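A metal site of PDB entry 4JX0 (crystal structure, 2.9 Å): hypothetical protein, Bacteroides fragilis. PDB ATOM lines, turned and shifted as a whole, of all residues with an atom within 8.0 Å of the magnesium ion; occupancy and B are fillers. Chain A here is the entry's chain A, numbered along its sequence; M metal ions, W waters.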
ATOM      1  N   ASN A 192     -12.033 -21.481  20.823  1.00  0.00           N
ATOM      2  CA  ASN A 192     -11.767 -22.912  21.066  1.00  0.00           C
ATOM      3  C   ASN A 192     -11.468 -23.290  22.541  1.00  0.00           C
ATOM      4  O   ASN A 192     -11.241 -24.472  22.784  1.00  0.00           O
ATOM      5  CB  ASN A 192     -10.622 -23.422  20.178  1.00  0.00           C
ATOM      6  CG  ASN A 192      -9.272 -22.823  20.412  1.00  0.00           C
ATOM      7  OD1 ASN A 192      -9.009 -22.138  21.420  1.00  0.00           O
ATOM      8  ND2 ASN A 192      -8.354 -23.096  19.486  1.00  0.00           N
ATOM      9  N   LYS A 205      -3.601 -37.138  23.177  1.00  0.00           N
ATOM     10  CA  LYS A 205      -2.928 -36.030  22.483  1.00  0.00           C
ATOM     11  C   LYS A 205      -3.918 -34.944  21.991  1.00  0.00           C
ATOM     12  O   LYS A 205      -3.498 -34.063  21.236  1.00  0.00           O
ATOM     13  CB  LYS A 205      -2.136 -36.582  21.291  1.00  0.00           C
ATOM     14  CG  LYS A 205      -1.120 -37.668  21.628  1.00  0.00           C
ATOM     15  CD  LYS A 205      -0.124 -37.234  22.695  1.00  0.00           C
ATOM     16  CE  LYS A 205       1.078 -38.155  22.781  1.00  0.00           C
ATOM     17  NZ  LYS A 205       1.840 -37.960  24.046  1.00  0.00           N
ATOM     18  N   LEU A 206      -5.188 -34.982  22.425  1.00  0.00           N
ATOM     19  CA  LEU A 206      -6.184 -34.002  21.928  1.00  0.00           C
ATOM     20  C   LEU A 206      -6.099 -32.632  22.617  1.00  0.00           C
ATOM     21  O   LEU A 206      -6.705 -31.689  22.112  1.00  0.00           O
ATOM     22  CB  LEU A 206      -7.615 -34.563  22.081  1.00  0.00           C
ATOM     23  CG  LEU A 206      -7.953 -35.804  21.235  1.00  0.00           C
ATOM     24  CD1 LEU A 206      -9.244 -36.412  21.685  1.00  0.00           C
ATOM     25  CD2 LEU A 206      -8.043 -35.474  19.765  1.00  0.00           C
ATOM     26  N   GLY A 207      -5.332 -32.503  23.707  1.00  0.00           N
ATOM     27  CA  GLY A 207      -5.151 -31.234  24.396  1.00  0.00           C
ATOM     28  C   GLY A 207      -4.460 -30.173  23.548  1.00  0.00           C
ATOM     29  O   GLY A 207      -4.657 -28.969  23.744  1.00  0.00           O
ATOM     30  N   SER A 208      -3.658 -30.632  22.559  1.00  0.00           N
ATOM     31  CA  SER A 208      -2.940 -29.791  21.619  1.00  0.00           C
ATOM     32  C   SER A 208      -3.866 -29.065  20.620  1.00  0.00           C
ATOM     33  O   SER A 208      -3.425 -28.129  19.955  1.00  0.00           O
ATOM     34  CB  SER A 208      -1.933 -30.622  20.832  1.00  0.00           C
ATOM     35  OG  SER A 208      -2.581 -31.544  19.969  1.00  0.00           O
ATOM     36  N   LEU A 209      -5.130 -29.525  20.459  1.00  0.00           N
ATOM     37  CA  LEU A 209      -6.043 -28.939  19.492  1.00  0.00           C
ATOM     38  C   LEU A 209      -6.588 -27.581  19.941  1.00  0.00           C
ATOM     39  O   LEU A 209      -7.139 -26.875  19.092  1.00  0.00           O
ATOM     40  CB  LEU A 209      -7.191 -29.906  19.171  1.00  0.00           C
ATOM     41  CG  LEU A 209      -6.777 -31.290  18.631  1.00  0.00           C
ATOM     42  CD1 LEU A 209      -7.979 -32.161  18.444  1.00  0.00           C
ATOM     43  CD2 LEU A 209      -6.021 -31.184  17.353  1.00  0.00           C
ATOM     44  N   ASN A 210      -6.434 -27.178  21.233  1.00  0.00           N
ATOM     45  CA  ASN A 210      -6.869 -25.858  21.693  1.00  0.00           C
ATOM     46  C   ASN A 210      -5.829 -25.210  22.652  1.00  0.00           C
ATOM     47  O   ASN A 210      -6.191 -24.343  23.444  1.00  0.00           O
ATOM     48  CB  ASN A 210      -8.264 -25.911  22.338  1.00  0.00           C
ATOM     49  CG  ASN A 210      -8.413 -26.777  23.558  1.00  0.00           C
ATOM     50  OD1 ASN A 210      -7.564 -27.628  23.874  1.00  0.00           O
ATOM     51  ND2 ASN A 210      -9.547 -26.621  24.233  1.00  0.00           N
ATOM     52  N   ASP A 211      -4.544 -25.560  22.499  1.00  0.00           N
ATOM     53  CA  ASP A 211      -3.442 -24.911  23.219  1.00  0.00           C
ATOM     54  C   ASP A 211      -3.107 -23.645  22.410  1.00  0.00           C
ATOM     55  O   ASP A 211      -3.806 -23.336  21.436  1.00  0.00           O
ATOM     56  CB  ASP A 211      -2.236 -25.857  23.391  1.00  0.00           C
ATOM     57  CG  ASP A 211      -1.510 -26.331  22.131  1.00  0.00           C
ATOM     58  OD1 ASP A 211      -1.875 -25.871  21.029  1.00  0.00           O
ATOM     59  OD2 ASP A 211      -0.582 -27.154  22.253  1.00  0.00           O
ATOM     60  N   GLY A 212      -2.062 -22.916  22.736  1.00  0.00           N
ATOM     61  CA  GLY A 212      -1.736 -21.736  21.928  1.00  0.00           C
ATOM     62  C   GLY A 212      -1.071 -22.041  20.594  1.00  0.00           C
ATOM     63  O   GLY A 212      -1.116 -21.224  19.680  1.00  0.00           O
ATOM     64  N   ASN A 213      -0.418 -23.219  20.489  1.00  0.00           N
ATOM     65  CA  ASN A 213       0.402 -23.621  19.358  1.00  0.00           C
ATOM     66  C   ASN A 213      -0.394 -24.054  18.142  1.00  0.00           C
ATOM     67  O   ASN A 213      -1.219 -24.964  18.221  1.00  0.00           O
ATOM     68  CB  ASN A 213       1.343 -24.758  19.762  1.00  0.00           C
ATOM     69  CG  ASN A 213       2.629 -24.753  18.995  1.00  0.00           C
ATOM     70  OD1 ASN A 213       2.663 -24.488  17.785  1.00  0.00           O
ATOM     71  ND2 ASN A 213       3.730 -25.089  19.658  1.00  0.00           N
ATOM     72  N   PHE A 214      -0.081 -23.426  16.984  1.00  0.00           N
ATOM     73  CA  PHE A 214      -0.689 -23.701  15.684  1.00  0.00           C
ATOM     74  C   PHE A 214       0.209 -24.534  14.764  1.00  0.00           C
ATOM     75  O   PHE A 214      -0.317 -25.172  13.859  1.00  0.00           O
ATOM     76  CB  PHE A 214      -0.985 -22.380  14.967  1.00  0.00           C
ATOM     77  CG  PHE A 214      -1.982 -21.489  15.666  1.00  0.00           C
ATOM     78  CD1 PHE A 214      -1.576 -20.603  16.637  1.00  0.00           C
ATOM     79  CD2 PHE A 214      -3.313 -21.491  15.288  1.00  0.00           C
ATOM     80  CE1 PHE A 214      -2.498 -19.765  17.258  1.00  0.00           C
ATOM     81  CE2 PHE A 214      -4.236 -20.653  15.909  1.00  0.00           C
ATOM     82  CZ  PHE A 214      -3.827 -19.805  16.897  1.00  0.00           C
ATOM     83  N   THR A 215       1.537 -24.510  14.951  1.00  0.00           N
ATOM     84  CA  THR A 215       2.496 -25.197  14.065  1.00  0.00           C
ATOM     85  C   THR A 215       3.028 -26.549  14.611  1.00  0.00           C
ATOM     86  O   THR A 215       3.569 -27.317  13.822  1.00  0.00           O
ATOM     87  CB  THR A 215       3.677 -24.262  13.814  1.00  0.00           C
ATOM     88  OG1 THR A 215       4.309 -23.947  15.065  1.00  0.00           O
ATOM     89  CG2 THR A 215       3.255 -22.971  13.116  1.00  0.00           C
ATOM     90  N   ALA A 216       2.883 -26.841  15.920  1.00  0.00           N
ATOM     91  CA  ALA A 216       3.374 -28.089  16.511  1.00  0.00           C
ATOM     92  C   ALA A 216       2.305 -29.183  16.465  1.00  0.00           C
ATOM     93  O   ALA A 216       1.145 -28.908  16.767  1.00  0.00           O
ATOM     94  CB  ALA A 216       3.800 -27.869  17.959  1.00  0.00           C
ATOM     95  N   ASN A 217       2.713 -30.421  16.148  1.00  0.00           N
ATOM     96  CA  ASN A 217       1.792 -31.536  16.039  1.00  0.00           C
ATOM     97  C   ASN A 217       1.974 -32.554  17.170  1.00  0.00           C
ATOM     98  O   ASN A 217       3.085 -32.855  17.600  1.00  0.00           O
ATOM     99  CB  ASN A 217       1.988 -32.251  14.719  1.00  0.00           C
ATOM    100  CG  ASN A 217       1.019 -33.379  14.523  1.00  0.00           C
ATOM    101  OD1 ASN A 217       1.358 -34.537  14.759  1.00  0.00           O
ATOM    102  ND2 ASN A 217      -0.219 -33.061  14.241  1.00  0.00           N
ATOM    103  N   ASN A 218       0.827 -33.111  17.600  1.00  0.00           N
ATOM    104  CA  ASN A 218       0.719 -34.193  18.576  1.00  0.00           C
ATOM    105  C   ASN A 218      -0.350 -35.202  18.124  1.00  0.00           C
ATOM    106  O   ASN A 218      -0.102 -36.407  18.196  1.00  0.00           O
ATOM    107  CB  ASN A 218       0.434 -33.647  19.974  1.00  0.00           C
ATOM    108  CG  ASN A 218       1.655 -33.050  20.617  1.00  0.00           C
ATOM    109  OD1 ASN A 218       2.616 -33.756  20.916  1.00  0.00           O
ATOM    110  ND2 ASN A 218       1.662 -31.739  20.832  1.00  0.00           N
ATOM    111  N   ASP A 244      -5.535 -26.235  11.581  1.00  0.00           N
ATOM    112  CA  ASP A 244      -4.120 -26.106  11.248  1.00  0.00           C
ATOM    113  C   ASP A 244      -3.582 -27.481  10.968  1.00  0.00           C
ATOM    114  O   ASP A 244      -3.760 -28.378  11.779  1.00  0.00           O
ATOM    115  CB  ASP A 244      -3.325 -25.429  12.367  1.00  0.00           C
ATOM    116  CG  ASP A 244      -3.577 -23.960  12.384  1.00  0.00           C
ATOM    117  OD1 ASP A 244      -4.702 -23.565  12.787  1.00  0.00           O
ATOM    118  OD2 ASP A 244      -2.718 -23.200  11.882  1.00  0.00           O
ATOM    119  N   VAL A 313      -3.580 -32.447  12.622  1.00  0.00           N
ATOM    120  CA  VAL A 313      -4.447 -31.356  13.041  1.00  0.00           C
ATOM    121  C   VAL A 313      -3.737 -30.803  14.262  1.00  0.00           C
ATOM    122  O   VAL A 313      -3.612 -31.484  15.273  1.00  0.00           O
ATOM    123  CB  VAL A 313      -5.942 -31.717  13.254  1.00  0.00           C
ATOM    124  CG1 VAL A 313      -6.745 -30.466  13.579  1.00  0.00           C
ATOM    125  CG2 VAL A 313      -6.516 -32.363  11.989  1.00  0.00           C
ATOM    126  N   ASN A 314      -3.109 -29.628  14.095  1.00  0.00           N
ATOM    127  CA  ASN A 314      -2.272 -28.962  15.087  1.00  0.00           C
ATOM    128  C   ASN A 314      -3.059 -28.037  15.996  1.00  0.00           C
ATOM    129  O   ASN A 314      -2.614 -27.750  17.110  1.00  0.00           O
ATOM    130  CB  ASN A 314      -1.190 -28.161  14.370  1.00  0.00           C
ATOM    131  CG  ASN A 314      -0.335 -28.978  13.425  1.00  0.00           C
ATOM    132  OD1 ASN A 314      -0.331 -30.200  13.488  1.00  0.00           O
ATOM    133  ND2 ASN A 314       0.366 -28.316  12.516  1.00  0.00           N
ATOM    134  N   GLU A 315      -4.206 -27.514  15.513  1.00  0.00           N
ATOM    135  CA  GLU A 315      -5.063 -26.591  16.255  1.00  0.00           C
ATOM    136  C   GLU A 315      -6.432 -26.533  15.556  1.00  0.00           C
ATOM    137  O   GLU A 315      -6.473 -26.578  14.335  1.00  0.00           O
ATOM    138  CB  GLU A 315      -4.402 -25.204  16.289  1.00  0.00           C
ATOM    139  CG  GLU A 315      -5.110 -24.158  17.120  1.00  0.00           C
ATOM    140  CD  GLU A 315      -4.910 -24.205  18.625  1.00  0.00           C
ATOM    141  OE1 GLU A 315      -4.222 -25.127  19.121  1.00  0.00           O
ATOM    142  OE2 GLU A 315      -5.454 -23.314  19.310  1.00  0.00           O
ATOM    143  N   VAL A 316      -7.528 -26.458  16.332  1.00  0.00           N
ATOM    144  CA  VAL A 316      -8.901 -26.371  15.807  1.00  0.00           C
ATOM    145  C   VAL A 316      -9.523 -25.089  16.340  1.00  0.00           C
ATOM    146  O   VAL A 316      -9.478 -24.862  17.550  1.00  0.00           O
ATOM    147  CB  VAL A 316      -9.758 -27.611  16.173  1.00  0.00           C
ATOM    148  CG1 VAL A 316     -11.179 -27.474  15.649  1.00  0.00           C
ATOM    149  CG2 VAL A 316      -9.127 -28.891  15.651  1.00  0.00           C
HETATM  150 MG    MG M   1      -2.327 -26.567  18.914  1.00  0.00          MG
HETATM  151  O   HOH W   1      -0.644 -27.944  18.841  1.00  0.00           O
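The magnesium ion is bound by the backbone carbonyl oxygen of Asn 213 (2.1 Å), the backbone carbonyl oxygen of Ser 208 (2.2 Å), water W1 (2.2 Å), the backbone carbonyl oxygen of Asn 314 (2.2 Å), the side-chain carboxylate of Asp 211 (2.3 Å) and the side-chain carboxylate of Glu 315 (2.4 Å).
Of the 20 residues printed, 5 come within 4 Å of the magnesium ion.
OD1 of Asn 213 lies within hydrogen-bond range of N of Ala 216 (3.0 Å).
The backbone NH of Thr 215 sits at hydrogen-bond distance from the side-chain amide oxygen of Asn 213, 3.0 Å away.
The side-chain hydroxyl (OG) of Ser 208 is in hydrogen-bond range of the backbone carbonyl oxygen (O) of Lys 205, 3.0 Å away.
The side-chain amide nitrogen (ND2) of Asn 314 sits close to the backbone carbonyl oxygen (O) of Phe 214 (3.5 Å).
The backbone carbonyl oxygen of Asp 244 lies within hydrogen-bond range of the backbone NH of Asn 314 (2.7 Å).
The side-chain amide nitrogen of Asn 217 is in hydrogen-bond range of the side-chain amide oxygen of Asn 314, at 3.0 Å.
The backbone NH (N) of Asp 244 is in hydrogen-bond range of the backbone carbonyl oxygen (O) of Glu 315, at 2.9 Å.
The side-chain amide nitrogen (ND2) of Asn 192 lies within hydrogen-bond range of the side-chain carboxylate (OE2) of Glu 315.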
